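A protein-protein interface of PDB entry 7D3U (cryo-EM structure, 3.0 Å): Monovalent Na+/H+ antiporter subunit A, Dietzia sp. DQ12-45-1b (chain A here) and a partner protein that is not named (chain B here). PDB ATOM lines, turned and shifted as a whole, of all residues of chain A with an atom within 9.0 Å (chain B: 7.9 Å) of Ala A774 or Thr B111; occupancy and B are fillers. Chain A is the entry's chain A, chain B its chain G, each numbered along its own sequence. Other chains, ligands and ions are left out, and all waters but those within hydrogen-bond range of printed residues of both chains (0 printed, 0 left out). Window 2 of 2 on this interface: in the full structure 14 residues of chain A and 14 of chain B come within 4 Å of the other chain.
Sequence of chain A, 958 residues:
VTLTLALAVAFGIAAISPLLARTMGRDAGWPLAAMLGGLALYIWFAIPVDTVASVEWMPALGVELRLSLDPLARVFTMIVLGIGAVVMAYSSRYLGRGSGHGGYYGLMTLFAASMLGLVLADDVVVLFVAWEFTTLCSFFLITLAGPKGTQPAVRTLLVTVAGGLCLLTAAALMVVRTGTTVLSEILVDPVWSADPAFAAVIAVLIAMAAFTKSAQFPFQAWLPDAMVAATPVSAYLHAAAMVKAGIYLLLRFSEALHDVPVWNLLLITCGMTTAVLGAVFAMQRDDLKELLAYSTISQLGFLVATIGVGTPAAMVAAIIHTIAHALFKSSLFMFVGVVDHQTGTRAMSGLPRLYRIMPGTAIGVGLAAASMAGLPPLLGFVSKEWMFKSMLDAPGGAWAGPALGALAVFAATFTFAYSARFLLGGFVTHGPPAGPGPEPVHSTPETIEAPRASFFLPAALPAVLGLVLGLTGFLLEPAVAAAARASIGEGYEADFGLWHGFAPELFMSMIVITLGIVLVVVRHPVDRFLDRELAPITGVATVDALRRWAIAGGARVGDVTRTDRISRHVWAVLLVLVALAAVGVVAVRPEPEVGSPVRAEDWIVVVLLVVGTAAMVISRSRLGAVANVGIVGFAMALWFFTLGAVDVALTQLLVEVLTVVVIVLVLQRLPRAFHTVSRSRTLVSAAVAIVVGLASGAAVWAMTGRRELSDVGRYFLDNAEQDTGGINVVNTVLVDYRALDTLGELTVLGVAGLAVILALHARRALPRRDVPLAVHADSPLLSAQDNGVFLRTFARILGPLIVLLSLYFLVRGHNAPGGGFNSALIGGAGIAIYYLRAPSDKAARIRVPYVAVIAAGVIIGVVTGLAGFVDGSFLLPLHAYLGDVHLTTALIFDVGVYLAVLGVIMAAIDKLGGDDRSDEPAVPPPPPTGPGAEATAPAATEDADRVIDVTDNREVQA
The backbone carbonyl oxygen of Ala A774 sits close to the backbone carbonyl oxygen of Phe B110, at 2.7 Å.
OD1 of Asp A778 lies within hydrogen-bond range of NE2 of His A776.
Among the printed residues, pairs that only touch across the chains: Leu A773 with Leu B94, Ala A774 with Thr B111, Val A775 with Phe B93, Val A775 with Leu B94 and His A776 with Glu B109.
Of chain B, only Phe B110 (2.7 Å) and Thr B111 (3.9 Å) come within 4 Å of Ala A774. Of the printed residues of chain B, Val A775 touches Phe B93 and Leu B94. Printed residues of chain A within 4 Å of Leu B94: Leu A773 and Val A775. Ser B95 touches none of the printed residues of chain A. Of the printed residues of chain A, Glu B109 touches His A776.
Hydrophobic or aromatic side chains of chain A that line the printed part of chain B: Leu A773, Val A775 and His A776. Hydrophobic or aromatic side chains of chain B that line the printed part of chain A: Phe B93 and Leu B94.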
ATOM      1  N   VAL A 771       9.622   6.750  37.921  1.00  0.00           N
ATOM      2  CA  VAL A 771       8.953   5.527  37.467  1.00  0.00           C
ATOM      3  C   VAL A 771       9.238   5.319  35.981  1.00  0.00           C
ATOM      4  O   VAL A 771       9.141   6.276  35.191  1.00  0.00           O
ATOM      5  CB  VAL A 771       7.446   5.599  37.757  1.00  0.00           C
ATOM      6  CG1 VAL A 771       6.751   6.654  36.902  1.00  0.00           C
ATOM      7  CG2 VAL A 771       6.801   4.235  37.546  1.00  0.00           C
ATOM      8  N   PRO A 772       9.652   4.126  35.564  1.00  0.00           N
ATOM      9  CA  PRO A 772       9.900   3.884  34.137  1.00  0.00           C
ATOM     10  C   PRO A 772       8.620   3.617  33.358  1.00  0.00           C
ATOM     11  O   PRO A 772       8.241   2.456  33.166  1.00  0.00           O
ATOM     12  CB  PRO A 772      10.822   2.659  34.144  1.00  0.00           C
ATOM     13  CG  PRO A 772      10.481   1.947  35.408  1.00  0.00           C
ATOM     14  CD  PRO A 772      10.105   3.006  36.407  1.00  0.00           C
ATOM     15  N   LEU A 773       7.936   4.678  32.930  1.00  0.00           N
ATOM     16  CA  LEU A 773       6.723   4.535  32.132  1.00  0.00           C
ATOM     17  C   LEU A 773       6.997   3.696  30.891  1.00  0.00           C
ATOM     18  O   LEU A 773       7.751   4.112  30.006  1.00  0.00           O
ATOM     19  CB  LEU A 773       6.171   5.905  31.738  1.00  0.00           C
ATOM     20  CG  LEU A 773       5.407   6.663  32.826  1.00  0.00           C
ATOM     21  CD1 LEU A 773       5.255   8.132  32.459  1.00  0.00           C
ATOM     22  CD2 LEU A 773       4.053   6.024  33.073  1.00  0.00           C
ATOM     23  N   ALA A 774       6.389   2.513  30.821  1.00  0.00           N
ATOM     24  CA  ALA A 774       6.659   1.567  29.738  1.00  0.00           C
ATOM     25  C   ALA A 774       5.664   1.756  28.592  1.00  0.00           C
ATOM     26  O   ALA A 774       4.934   0.847  28.199  1.00  0.00           O
ATOM     27  CB  ALA A 774       6.630   0.139  30.270  1.00  0.00           C
ATOM     28  N   VAL A 775       5.649   2.974  28.058  1.00  0.00           N
ATOM     29  CA  VAL A 775       4.866   3.320  26.875  1.00  0.00           C
ATOM     30  C   VAL A 775       5.711   4.242  26.008  1.00  0.00           C
ATOM     31  O   VAL A 775       6.439   5.097  26.522  1.00  0.00           O
ATOM     32  CB  VAL A 775       3.519   3.982  27.238  1.00  0.00           C
ATOM     33  CG1 VAL A 775       2.626   3.013  27.991  1.00  0.00           C
ATOM     34  CG2 VAL A 775       3.743   5.238  28.064  1.00  0.00           C
ATOM     35  N   HIS A 776       5.631   4.058  24.694  1.00  0.00           N
ATOM     36  CA  HIS A 776       6.444   4.880  23.814  1.00  0.00           C
ATOM     37  C   HIS A 776       5.793   6.248  23.609  1.00  0.00           C
ATOM     38  O   HIS A 776       4.637   6.482  23.970  1.00  0.00           O
ATOM     39  CB  HIS A 776       6.694   4.169  22.484  1.00  0.00           C
ATOM     40  CG  HIS A 776       5.467   3.969  21.653  1.00  0.00           C
ATOM     41  ND1 HIS A 776       4.941   2.722  21.396  1.00  0.00           N
ATOM     42  CD2 HIS A 776       4.678   4.853  20.997  1.00  0.00           C
ATOM     43  CE1 HIS A 776       3.873   2.846  20.629  1.00  0.00           C
ATOM     44  NE2 HIS A 776       3.691   4.129  20.373  1.00  0.00           N
ATOM     45  N   ALA A 777       6.565   7.162  23.017  1.00  0.00           N
ATOM     46  CA  ALA A 777       6.203   8.575  23.036  1.00  0.00           C
ATOM     47  C   ALA A 777       4.991   8.865  22.159  1.00  0.00           C
ATOM     48  O   ALA A 777       4.066   9.572  22.578  1.00  0.00           O
ATOM     49  CB  ALA A 777       7.396   9.423  22.598  1.00  0.00           C
ATOM     50  N   ASP A 778       4.971   8.331  20.941  1.00  0.00           N
ATOM     51  CA  ASP A 778       3.959   8.711  19.963  1.00  0.00           C
ATOM     52  C   ASP A 778       2.591   8.102  20.242  1.00  0.00           C
ATOM     53  O   ASP A 778       1.707   8.193  19.384  1.00  0.00           O
ATOM     54  CB  ASP A 778       4.417   8.325  18.552  1.00  0.00           C
ATOM     55  CG  ASP A 778       4.688   6.840  18.409  1.00  0.00           C
ATOM     56  OD1 ASP A 778       3.716   6.061  18.305  1.00  0.00           O
ATOM     57  OD2 ASP A 778       5.874   6.450  18.396  1.00  0.00           O
ATOM     58  N   SER A 779       2.394   7.494  21.401  1.00  0.00           N
ATOM     59  CA  SER A 779       1.095   6.893  21.646  1.00  0.00           C
ATOM     60  C   SER A 779       0.228   7.806  22.502  1.00  0.00           C
ATOM     61  O   SER A 779       0.742   8.612  23.283  1.00  0.00           O
ATOM     62  CB  SER A 779       1.248   5.542  22.352  1.00  0.00           C
ATOM     63  OG  SER A 779       1.012   5.668  23.743  1.00  0.00           O
ATOM     64  N   LEU A 782      -0.778   9.701  26.873  1.00  0.00           N
ATOM     65  CA  LEU A 782       0.333  10.517  27.340  1.00  0.00           C
ATOM     66  C   LEU A 782       0.002  11.963  27.003  1.00  0.00           C
ATOM     67  O   LEU A 782      -1.142  12.259  26.643  1.00  0.00           O
ATOM     68  CB  LEU A 782       1.652  10.082  26.698  1.00  0.00           C
ATOM     69  CG  LEU A 782       2.605   9.306  27.600  1.00  0.00           C
ATOM     70  CD1 LEU A 782       3.927   9.081  26.893  1.00  0.00           C
ATOM     71  CD2 LEU A 782       2.814  10.061  28.895  1.00  0.00           C
ATOM     72  N   PHE B  93      -2.972   1.773  32.652  1.00  0.00           N
ATOM     73  CA  PHE B  93      -2.272   1.566  31.390  1.00  0.00           C
ATOM     74  C   PHE B  93      -0.858   2.126  31.459  1.00  0.00           C
ATOM     75  O   PHE B  93       0.104   1.473  31.039  1.00  0.00           O
ATOM     76  CB  PHE B  93      -3.047   2.211  30.242  1.00  0.00           C
ATOM     77  CG  PHE B  93      -2.357   2.105  28.912  1.00  0.00           C
ATOM     78  CD1 PHE B  93      -1.407   3.036  28.527  1.00  0.00           C
ATOM     79  CD2 PHE B  93      -2.660   1.073  28.045  1.00  0.00           C
ATOM     80  CE1 PHE B  93      -0.777   2.941  27.308  1.00  0.00           C
ATOM     81  CE2 PHE B  93      -2.031   0.974  26.825  1.00  0.00           C
ATOM     82  CZ  PHE B  93      -1.086   1.907  26.459  1.00  0.00           C
ATOM     83  N   LEU B  94      -0.716   3.345  31.979  1.00  0.00           N
ATOM     84  CA  LEU B  94       0.604   3.958  32.071  1.00  0.00           C
ATOM     85  C   LEU B  94       1.508   3.193  33.028  1.00  0.00           C
ATOM     86  O   LEU B  94       2.687   2.972  32.733  1.00  0.00           O
ATOM     87  CB  LEU B  94       0.477   5.416  32.502  1.00  0.00           C
ATOM     88  CG  LEU B  94      -0.054   6.370  31.435  1.00  0.00           C
ATOM     89  CD1 LEU B  94       0.118   7.810  31.874  1.00  0.00           C
ATOM     90  CD2 LEU B  94       0.650   6.124  30.116  1.00  0.00           C
ATOM     91  N   SER B  95       0.976   2.776  34.179  1.00  0.00           N
ATOM     92  CA  SER B  95       1.791   2.054  35.147  1.00  0.00           C
ATOM     93  C   SER B  95       2.139   0.647  34.679  1.00  0.00           C
ATOM     94  O   SER B  95       3.035   0.022  35.255  1.00  0.00           O
ATOM     95  CB  SER B  95       1.076   1.989  36.494  1.00  0.00           C
ATOM     96  OG  SER B  95       1.836   1.249  37.433  1.00  0.00           O
ATOM     97  N   GLY B  96       1.456   0.136  33.660  1.00  0.00           N
ATOM     98  CA  GLY B  96       1.783  -1.167  33.118  1.00  0.00           C
ATOM     99  C   GLY B  96       0.812  -2.268  33.488  1.00  0.00           C
ATOM    100  O   GLY B  96       1.226  -3.405  33.731  1.00  0.00           O
ATOM    101  N   PRO B  99      -3.107  -6.139  29.976  1.00  0.00           N
ATOM    102  CA  PRO B  99      -4.454  -6.538  29.566  1.00  0.00           C
ATOM    103  C   PRO B  99      -4.584  -8.052  29.531  1.00  0.00           C
ATOM    104  O   PRO B  99      -3.604  -8.786  29.392  1.00  0.00           O
ATOM    105  CB  PRO B  99      -4.595  -5.934  28.167  1.00  0.00           C
ATOM    106  CG  PRO B  99      -3.199  -5.849  27.666  1.00  0.00           C
ATOM    107  CD  PRO B  99      -2.346  -5.543  28.866  1.00  0.00           C
ATOM    108  N   ILE B 108      -3.706   0.028  20.413  1.00  0.00           N
ATOM    109  CA  ILE B 108      -2.855   0.826  21.285  1.00  0.00           C
ATOM    110  C   ILE B 108      -1.731  -0.072  21.774  1.00  0.00           C
ATOM    111  O   ILE B 108      -1.990  -1.115  22.387  1.00  0.00           O
ATOM    112  CB  ILE B 108      -3.634   1.410  22.474  1.00  0.00           C
ATOM    113  CG1 ILE B 108      -4.692   2.391  21.981  1.00  0.00           C
ATOM    114  CG2 ILE B 108      -2.694   2.110  23.424  1.00  0.00           C
ATOM    115  CD1 ILE B 108      -4.108   3.594  21.308  1.00  0.00           C
ATOM    116  N   GLU B 109      -0.491   0.325  21.508  1.00  0.00           N
ATOM    117  CA  GLU B 109       0.644  -0.498  21.894  1.00  0.00           C
ATOM    118  C   GLU B 109       0.889  -0.408  23.395  1.00  0.00           C
ATOM    119  O   GLU B 109       0.619   0.612  24.033  1.00  0.00           O
ATOM    120  CB  GLU B 109       1.896  -0.074  21.130  1.00  0.00           C
ATOM    121  CG  GLU B 109       1.786  -0.234  19.623  1.00  0.00           C
ATOM    122  CD  GLU B 109       1.684  -1.685  19.189  1.00  0.00           C
ATOM    123  OE1 GLU B 109       0.586  -2.272  19.300  1.00  0.00           O
ATOM    124  OE2 GLU B 109       2.706  -2.240  18.736  1.00  0.00           O
ATOM    125  N   PHE B 110       1.411  -1.493  23.957  1.00  0.00           N
ATOM    126  CA  PHE B 110       1.649  -1.598  25.391  1.00  0.00           C
ATOM    127  C   PHE B 110       3.122  -1.605  25.763  1.00  0.00           C
ATOM    128  O   PHE B 110       3.494  -1.002  26.770  1.00  0.00           O
ATOM    129  CB  PHE B 110       0.985  -2.864  25.941  1.00  0.00           C
ATOM    130  CG  PHE B 110      -0.504  -2.756  26.071  1.00  0.00           C
ATOM    131  CD1 PHE B 110      -1.328  -3.014  24.989  1.00  0.00           C
ATOM    132  CD2 PHE B 110      -1.082  -2.395  27.276  1.00  0.00           C
ATOM    133  CE1 PHE B 110      -2.700  -2.915  25.108  1.00  0.00           C
ATOM    134  CE2 PHE B 110      -2.453  -2.296  27.398  1.00  0.00           C
ATOM    135  CZ  PHE B 110      -3.263  -2.555  26.313  1.00  0.00           C
ATOM    136  N   THR B 111       3.961  -2.280  24.980  1.00  0.00           N
ATOM    137  CA  THR B 111       5.402  -2.344  25.220  1.00  0.00           C
ATOM    138  C   THR B 111       5.733  -2.832  26.630  1.00  0.00           C
ATOM    139  O   THR B 111       4.974  -3.592  27.230  1.00  0.00           O
ATOM    140  CB  THR B 111       6.074  -0.974  24.995  1.00  0.00           C
ATOM    141  OG1 THR B 111       6.030  -0.641  23.602  1.00  0.00           O
ATOM    142  CG2 THR B 111       7.521  -1.004  25.460  1.00  0.00           C
